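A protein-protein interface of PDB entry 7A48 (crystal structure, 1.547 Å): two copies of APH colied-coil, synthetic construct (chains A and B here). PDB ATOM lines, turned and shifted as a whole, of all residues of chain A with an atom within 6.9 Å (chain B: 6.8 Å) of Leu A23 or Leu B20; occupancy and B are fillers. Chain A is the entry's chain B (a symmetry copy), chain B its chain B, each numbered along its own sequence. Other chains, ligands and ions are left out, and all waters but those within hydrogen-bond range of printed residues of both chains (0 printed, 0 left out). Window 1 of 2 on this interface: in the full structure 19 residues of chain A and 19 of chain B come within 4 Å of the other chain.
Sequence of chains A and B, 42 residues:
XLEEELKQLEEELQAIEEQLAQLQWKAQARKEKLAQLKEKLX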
ATOM      1  N   GLU A  18      20.384 -23.753  10.395  1.00  0.00           N
ATOM      2  CA  GLU A  18      21.100 -23.046   9.337  1.00  0.00           C
ATOM      3  C   GLU A  18      20.231 -22.887   8.091  1.00  0.00           C
ATOM      4  O   GLU A  18      20.205 -21.811   7.480  1.00  0.00           O
ATOM      5  CB  GLU A  18      22.392 -23.797   8.996  1.00  0.00           C
ATOM      6  CG  GLU A  18      23.522 -23.605   9.993  1.00  0.00           C
ATOM      7  CD  GLU A  18      24.629 -24.621   9.823  1.00  0.00           C
ATOM      8  OE1 GLU A  18      24.434 -25.607   9.083  1.00  0.00           O
ATOM      9  OE2 GLU A  18      25.700 -24.437  10.442  1.00  0.00           O
ATOM     10  N   GLN A  19      19.537 -23.957   7.686  1.00  0.00           N
ATOM     11  CA  GLN A  19      18.634 -23.875   6.538  1.00  0.00           C
ATOM     12  C   GLN A  19      17.461 -22.946   6.822  1.00  0.00           C
ATOM     13  O   GLN A  19      17.015 -22.204   5.930  1.00  0.00           O
ATOM     14  CB  GLN A  19      18.119 -25.265   6.169  1.00  0.00           C
ATOM     15  CG  GLN A  19      19.172 -26.217   5.659  1.00  0.00           C
ATOM     16  CD  GLN A  19      18.622 -27.615   5.507  1.00  0.00           C
ATOM     17  OE1 GLN A  19      17.638 -27.827   4.801  1.00  0.00           O
ATOM     18  NE2 GLN A  19      19.235 -28.573   6.192  1.00  0.00           N
ATOM     19  N   LEU A  20      16.951 -22.985   8.057  1.00  0.00           N
ATOM     20  CA  LEU A  20      15.869 -22.096   8.474  1.00  0.00           C
ATOM     21  C   LEU A  20      16.280 -20.634   8.340  1.00  0.00           C
ATOM     22  O   LEU A  20      15.545 -19.817   7.774  1.00  0.00           O
ATOM     23  CB  LEU A  20      15.471 -22.451   9.917  1.00  0.00           C
ATOM     24  CG  LEU A  20      14.228 -21.889  10.612  1.00  0.00           C
ATOM     25  CD1 LEU A  20      13.887 -22.770  11.807  1.00  0.00           C
ATOM     26  CD2 LEU A  20      14.482 -20.485  11.072  1.00  0.00           C
ATOM     27  N   ALA A  21      17.456 -20.290   8.831  1.00  0.00           N
ATOM     28  CA  ALA A  21      17.921 -18.915   8.722  1.00  0.00           C
ATOM     29  C   ALA A  21      18.074 -18.500   7.260  1.00  0.00           C
ATOM     30  O   ALA A  21      17.825 -17.368   6.899  1.00  0.00           O
ATOM     31  CB  ALA A  21      19.236 -18.745   9.457  1.00  0.00           C
ATOM     32  N   GLN A  22      18.498 -19.430   6.422  1.00  0.00           N
ATOM     33  CA  GLN A  22      18.657 -19.125   5.012  1.00  0.00           C
ATOM     34  C   GLN A  22      17.315 -18.763   4.396  1.00  0.00           C
ATOM     35  O   GLN A  22      17.229 -17.847   3.610  1.00  0.00           O
ATOM     36  CB  GLN A  22      19.298 -20.281   4.251  1.00  0.00           C
ATOM     37  CG  GLN A  22      19.672 -19.899   2.833  1.00  0.00           C
ATOM     38  CD  GLN A  22      20.036 -21.067   1.950  1.00  0.00           C
ATOM     39  OE1 GLN A  22      20.046 -20.944   0.736  1.00  0.00           O
ATOM     40  NE2 GLN A  22      20.353 -22.196   2.553  1.00  0.00           N
ATOM     41  N   LEU A  23      16.274 -19.502   4.752  1.00  0.00           N
ATOM     42  CA  LEU A  23      14.949 -19.220   4.225  1.00  0.00           C
ATOM     43  C   LEU A  23      14.373 -17.924   4.786  1.00  0.00           C
ATOM     44  O   LEU A  23      13.623 -17.252   4.117  1.00  0.00           O
ATOM     45  CB  LEU A  23      13.993 -20.386   4.473  1.00  0.00           C
ATOM     46  CG  LEU A  23      14.290 -21.654   3.684  1.00  0.00           C
ATOM     47  CD1 LEU A  23      13.294 -22.745   4.045  1.00  0.00           C
ATOM     48  CD2 LEU A  23      14.269 -21.390   2.194  1.00  0.00           C
ATOM     49  N   GLN A  24      14.728 -17.581   6.016  1.00  0.00           N
ATOM     50  CA  GLN A  24      14.254 -16.338   6.611  1.00  0.00           C
ATOM     51  C   GLN A  24      14.833 -15.161   5.834  1.00  0.00           C
ATOM     52  O   GLN A  24      14.157 -14.198   5.566  1.00  0.00           O
ATOM     53  CB  GLN A  24      14.645 -16.245   8.082  1.00  0.00           C
ATOM     54  CG  GLN A  24      13.824 -17.153   8.978  1.00  0.00           C
ATOM     55  CD  GLN A  24      14.294 -17.167  10.412  1.00  0.00           C
ATOM     56  OE1 GLN A  24      15.477 -17.031  10.694  1.00  0.00           O
ATOM     57  NE2 GLN A  24      13.371 -17.381  11.323  1.00  0.00           N
ATOM     58  N   TRP A  25      16.106 -15.274   5.490  1.00  0.00           N
ATOM     59  CA  TRP A  25      16.803 -14.269   4.711  1.00  0.00           C
ATOM     60  C   TRP A  25      16.111 -14.092   3.358  1.00  0.00           C
ATOM     61  O   TRP A  25      15.789 -12.993   2.965  1.00  0.00           O
ATOM     62  CB  TRP A  25      18.259 -14.719   4.561  1.00  0.00           C
ATOM     63  CG  TRP A  25      19.076 -14.076   3.493  1.00  0.00           C
ATOM     64  CD1 TRP A  25      19.344 -12.757   3.348  1.00  0.00           C
ATOM     65  CD2 TRP A  25      19.781 -14.745   2.448  1.00  0.00           C
ATOM     66  NE1 TRP A  25      20.150 -12.558   2.263  1.00  0.00           N
ATOM     67  CE2 TRP A  25      20.434 -13.766   1.692  1.00  0.00           C
ATOM     68  CE3 TRP A  25      19.905 -16.077   2.066  1.00  0.00           C
ATOM     69  CZ2 TRP A  25      21.199 -14.077   0.584  1.00  0.00           C
ATOM     70  CZ3 TRP A  25      20.665 -16.380   0.968  1.00  0.00           C
ATOM     71  CH2 TRP A  25      21.302 -15.387   0.239  1.00  0.00           C
ATOM     72  N   LYS A  26      15.862 -15.192   2.668  1.00  0.00           N
ATOM     73  CA  LYS A  26      15.205 -15.148   1.369  1.00  0.00           C
ATOM     74  C   LYS A  26      13.783 -14.607   1.421  1.00  0.00           C
ATOM     75  O   LYS A  26      13.359 -13.889   0.544  1.00  0.00           O
ATOM     76  CB  LYS A  26      15.201 -16.531   0.737  1.00  0.00           C
ATOM     77  CG  LYS A  26      16.589 -17.026   0.416  1.00  0.00           C
ATOM     78  CD  LYS A  26      16.550 -18.192  -0.532  1.00  0.00           C
ATOM     79  CE  LYS A  26      17.945 -18.501  -1.029  1.00  0.00           C
ATOM     80  NZ  LYS A  26      17.946 -19.483  -2.143  1.00  0.00           N
ATOM     81  N   ALA A  27      13.054 -14.962   2.464  1.00  0.00           N
ATOM     82  CA  ALA A  27      11.686 -14.500   2.604  1.00  0.00           C
ATOM     83  C   ALA A  27      11.622 -12.999   2.879  1.00  0.00           C
ATOM     84  O   ALA A  27      10.873 -12.285   2.248  1.00  0.00           O
ATOM     85  CB  ALA A  27      10.975 -15.281   3.693  1.00  0.00           C
ATOM     86  N   GLN A  28      12.446 -12.518   3.797  1.00  0.00           N
ATOM     87  CA  GLN A  28      12.457 -11.101   4.134  1.00  0.00           C
ATOM     88  C   GLN A  28      12.890 -10.229   2.959  1.00  0.00           C
ATOM     89  O   GLN A  28      12.390  -9.142   2.775  1.00  0.00           O
ATOM     90  CB  GLN A  28      13.339 -10.846   5.356  1.00  0.00           C
ATOM     91  CG  GLN A  28      13.341  -9.414   5.861  1.00  0.00           C
ATOM     92  CD  GLN A  28      11.968  -8.912   6.258  1.00  0.00           C
ATOM     93  OE1 GLN A  28      11.078  -9.680   6.540  1.00  0.00           O
ATOM     94  NE2 GLN A  28      11.808  -7.606   6.280  1.00  0.00           N
ATOM     95  N   ALA A  29      13.812 -10.735   2.154  1.00  0.00           N
ATOM     96  CA  ALA A  29      14.283 -10.010   0.992  1.00  0.00           C
ATOM     97  C   ALA A  29      13.151  -9.774  -0.006  1.00  0.00           C
ATOM     98  O   ALA A  29      13.068  -8.728  -0.616  1.00  0.00           O
ATOM     99  CB  ALA A  29      15.424 -10.761   0.341  1.00  0.00           C
ATOM    100  N   LYS A  31       9.905  -9.802   0.816  1.00  0.00           N
ATOM    101  CA  LYS A  31       8.911  -8.954   1.440  1.00  0.00           C
ATOM    102  C   LYS A  31       9.293  -7.500   1.208  1.00  0.00           C
ATOM    103  O   LYS A  31       8.439  -6.670   0.941  1.00  0.00           O
ATOM    104  CB  LYS A  31       8.799  -9.239   2.939  1.00  0.00           C
ATOM    105  CG  LYS A  31       8.066 -10.523   3.265  1.00  0.00           C
ATOM    106  CD  LYS A  31       8.123 -10.842   4.746  1.00  0.00           C
ATOM    107  CE  LYS A  31       7.665 -12.268   4.997  1.00  0.00           C
ATOM    108  NZ  LYS A  31       7.705 -12.620   6.433  1.00  0.00           N
ATOM    109  N   ALA B  15       5.737 -19.659  -1.295  1.00  0.00           N
ATOM    110  CA  ALA B  15       6.357 -20.975  -1.404  1.00  0.00           C
ATOM    111  C   ALA B  15       7.541 -21.095  -0.453  1.00  0.00           C
ATOM    112  O   ALA B  15       7.687 -22.116   0.235  1.00  0.00           O
ATOM    113  CB  ALA B  15       6.798 -21.235  -2.847  1.00  0.00           C
ATOM    114  N   ILE B  16       8.381 -20.056  -0.385  1.00  0.00           N
ATOM    115  CA  ILE B  16       9.490 -20.032   0.567  1.00  0.00           C
ATOM    116  C   ILE B  16       8.956 -20.089   1.991  1.00  0.00           C
ATOM    117  O   ILE B  16       9.504 -20.790   2.855  1.00  0.00           O
ATOM    118  CB  ILE B  16      10.371 -18.788   0.349  1.00  0.00           C
ATOM    119  CG1 ILE B  16      11.101 -18.868  -0.990  1.00  0.00           C
ATOM    120  CG2 ILE B  16      11.396 -18.637   1.457  1.00  0.00           C
ATOM    121  CD1 ILE B  16      11.613 -17.527  -1.472  1.00  0.00           C
ATOM    122  N   GLU B  17       7.861 -19.369   2.255  1.00  0.00           N
ATOM    123  CA  GLU B  17       7.295 -19.345   3.602  1.00  0.00           C
ATOM    124  C   GLU B  17       6.768 -20.715   4.028  1.00  0.00           C
ATOM    125  O   GLU B  17       6.830 -21.066   5.212  1.00  0.00           O
ATOM    126  CB  GLU B  17       6.184 -18.298   3.668  1.00  0.00           C
ATOM    127  CG  GLU B  17       6.675 -16.862   3.654  1.00  0.00           C
ATOM    128  CD  GLU B  17       6.932 -16.326   5.049  1.00  0.00           C
ATOM    129  OE1 GLU B  17       7.083 -17.139   5.984  1.00  0.00           O
ATOM    130  OE2 GLU B  17       6.970 -15.092   5.212  1.00  0.00           O
ATOM    131  N   GLU B  18       6.213 -21.485   3.085  1.00  0.00           N
ATOM    132  CA  GLU B  18       5.789 -22.853   3.372  1.00  0.00           C
ATOM    133  C   GLU B  18       6.974 -23.724   3.785  1.00  0.00           C
ATOM    134  O   GLU B  18       6.870 -24.509   4.737  1.00  0.00           O
ATOM    135  CB  GLU B  18       5.093 -23.446   2.142  1.00  0.00           C
ATOM    136  CG  GLU B  18       3.666 -22.970   1.927  1.00  0.00           C
ATOM    137  CD  GLU B  18       3.149 -23.284   0.541  1.00  0.00           C
ATOM    138  OE1 GLU B  18       3.953 -23.675  -0.328  1.00  0.00           O
ATOM    139  OE2 GLU B  18       1.928 -23.129   0.317  1.00  0.00           O
ATOM    140  N   GLN B  19       8.095 -23.619   3.063  1.00  0.00           N
ATOM    141  CA  GLN B  19       9.295 -24.373   3.426  1.00  0.00           C
ATOM    142  C   GLN B  19       9.853 -23.912   4.766  1.00  0.00           C
ATOM    143  O   GLN B  19      10.334 -24.734   5.564  1.00  0.00           O
ATOM    144  CB  GLN B  19      10.361 -24.227   2.342  1.00  0.00           C
ATOM    145  CG  GLN B  19      10.004 -24.847   1.014  1.00  0.00           C
ATOM    146  CD  GLN B  19      11.015 -24.489  -0.049  1.00  0.00           C
ATOM    147  OE1 GLN B  19      12.207 -24.747   0.108  1.00  0.00           O
ATOM    148  NE2 GLN B  19      10.550 -23.866  -1.126  1.00  0.00           N
ATOM    149  N   LEU B  20       9.800 -22.600   5.019  1.00  0.00           N
ATOM    150  CA  LEU B  20      10.241 -22.041   6.294  1.00  0.00           C
ATOM    151  C   LEU B  20       9.441 -22.625   7.453  1.00  0.00           C
ATOM    152  O   LEU B  20      10.010 -23.067   8.459  1.00  0.00           O
ATOM    153  CB  LEU B  20      10.117 -20.509   6.227  1.00  0.00           C
ATOM    154  CG  LEU B  20      10.695 -19.568   7.287  1.00  0.00           C
ATOM    155  CD1 LEU B  20      10.805 -18.166   6.701  1.00  0.00           C
ATOM    156  CD2 LEU B  20       9.809 -19.544   8.496  1.00  0.00           C
ATOM    157  N   ALA B  21       8.128 -22.660   7.325  1.00  0.00           N
ATOM    158  CA  ALA B  21       7.303 -23.221   8.384  1.00  0.00           C
ATOM    159  C   ALA B  21       7.620 -24.699   8.604  1.00  0.00           C
ATOM    160  O   ALA B  21       7.586 -25.190   9.714  1.00  0.00           O
ATOM    161  CB  ALA B  21       5.834 -23.042   8.057  1.00  0.00           C
ATOM    162  N   GLN B  22       7.922 -25.406   7.529  1.00  0.00           N
ATOM    163  CA  GLN B  22       8.251 -26.814   7.649  1.00  0.00           C
ATOM    164  C   GLN B  22       9.510 -26.992   8.481  1.00  0.00           C
ATOM    165  O   GLN B  22       9.584 -27.880   9.299  1.00  0.00           O
ATOM    166  CB  GLN B  22       8.414 -27.477   6.285  1.00  0.00           C
ATOM    167  CG  GLN B  22       8.539 -28.984   6.389  1.00  0.00           C
ATOM    168  CD  GLN B  22       8.991 -29.659   5.118  1.00  0.00           C
ATOM    169  OE1 GLN B  22       9.430 -30.796   5.146  1.00  0.00           O
ATOM    170  NE2 GLN B  22       8.869 -28.971   4.000  1.00  0.00           N
ATOM    171  N   LEU B  23      10.504 -26.146   8.251  1.00  0.00           N
ATOM    172  CA  LEU B  23      11.742 -26.230   9.009  1.00  0.00           C
ATOM    173  C   LEU B  23      11.555 -25.803  10.461  1.00  0.00           C
ATOM    174  O   LEU B  23      12.228 -26.302  11.332  1.00  0.00           O
ATOM    175  CB  LEU B  23      12.854 -25.417   8.347  1.00  0.00           C
ATOM    176  CG  LEU B  23      13.360 -25.963   7.018  1.00  0.00           C
ATOM    177  CD1 LEU B  23      14.434 -25.049   6.449  1.00  0.00           C
ATOM    178  CD2 LEU B  23      13.888 -27.372   7.168  1.00  0.00           C
ATOM    179  N   GLN B  24      10.639 -24.879  10.712  1.00  0.00           N
ATOM    180  CA  GLN B  24      10.371 -24.444  12.077  1.00  0.00           C
ATOM    181  C   GLN B  24       9.787 -25.611  12.865  1.00  0.00           C
ATOM    182  O   GLN B  24      10.135 -25.834  13.999  1.00  0.00           O
ATOM    183  CB  GLN B  24       9.413 -23.258  12.101  1.00  0.00           C
ATOM    184  CG  GLN B  24      10.061 -21.958  11.664  1.00  0.00           C
ATOM    185  CD  GLN B  24       9.088 -20.809  11.556  1.00  0.00           C
ATOM    186  OE1 GLN B  24       7.925 -20.990  11.221  1.00  0.00           O
ATOM    187  NE2 GLN B  24       9.576 -19.611  11.794  1.00  0.00           N
ATOM    188  N   TRP B  25       8.887 -26.341  12.225  1.00  0.00           N
ATOM    189  CA  TRP B  25       8.264 -27.512  12.810  1.00  0.00           C
ATOM    190  C   TRP B  25       9.335 -28.547  13.161  1.00  0.00           C
ATOM    191  O   TRP B  25       9.388 -29.035  14.267  1.00  0.00           O
ATOM    192  CB  TRP B  25       7.247 -28.054  11.801  1.00  0.00           C
ATOM    193  CG  TRP B  25       6.764 -29.452  11.987  1.00  0.00           C
ATOM    194  CD1 TRP B  25       6.139 -29.966  13.071  1.00  0.00           C
ATOM    195  CD2 TRP B  25       6.821 -30.502  11.022  1.00  0.00           C
ATOM    196  NE1 TRP B  25       5.826 -31.279  12.856  1.00  0.00           N
ATOM    197  CE2 TRP B  25       6.234 -31.633  11.602  1.00  0.00           C
ATOM    198  CE3 TRP B  25       7.330 -30.602   9.732  1.00  0.00           C
ATOM    199  CZ2 TRP B  25       6.141 -32.839  10.935  1.00  0.00           C
ATOM    200  CZ3 TRP B  25       7.234 -31.800   9.075  1.00  0.00           C
ATOM    201  CH2 TRP B  25       6.646 -32.903   9.675  1.00  0.00           C
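Hydrophobic or aromatic side chains of chain A within 4 Å of the printed part of chain B: Leu A20 and Leu A23. Among the printed residues, 9 pairs touch across the chains. Among the printed residues, Asp or Glu carboxylates within 4 Å of a Lys or Arg side-chain nitrogen of the other chain: Lys A31 with Glu B17.
Gln A19 touches Leu B23, and with the chains exchanged Leu A23 touches Gln B19. Leu A20 touches Leu B23, and with the chains exchanged Leu A23 touches Leu B20. Leu A20 touches Gln B24, and with the chains exchanged Gln A24 touches Leu B20. Leu B23 touches its own counterpart, Leu A23. Positions printed for both chains: 18, 19, 20, 21, 22, 23, 24 and 25. Of the 9 pairs that touch across the chains among the printed residues, 7 have their exchanged pair printed and touching as well.
The side-chain carboxylate of Glu B17 is in salt-bridge range of the side-chain amino group of Lys A31, 2.9 Å away.
Printed residues of chain B within 4 Å of Gln A19: Leu B23 (3.7 Å). Of the printed residues of chain B, Leu A20 touches Leu B23 and Gln B24. Of chain B, only Ile B16, Gln B19, Leu B20 and Leu B23 come within 4 Å of Leu A23. Printed residues of chain A within 4 Å of Ile B16: Leu A23 (3.7 Å). Of the printed residues of chain A, Glu B17 touches Lys A31 (2.9 Å). Leu B20 touches just these residues of chain A: Leu A23 (3.6 Å) and Gln A24 (3.9 Å). The nearest residue of chain B that does not touch Leu A23 is Ala B21 (6.1 Å). The nearest printed residue of chain A that does not touch Glu B17 is Ala A27 (4.3 Å).
Among the printed residues, pairs that only touch across the chains: Gln A19 with Leu B23 (3.7 Å), Leu A20 with Leu B23 (3.6 Å), Leu A20 with Gln B24 (3.9 Å), Leu A23 with Ile B16 (3.7 Å), Leu A23 with Gln B19 (3.7 Å), Leu A23 with Leu B20 (3.6 Å), Leu A23 with Leu B23 (3.5 Å) and Gln A24 with Leu B20 (3.9 Å).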
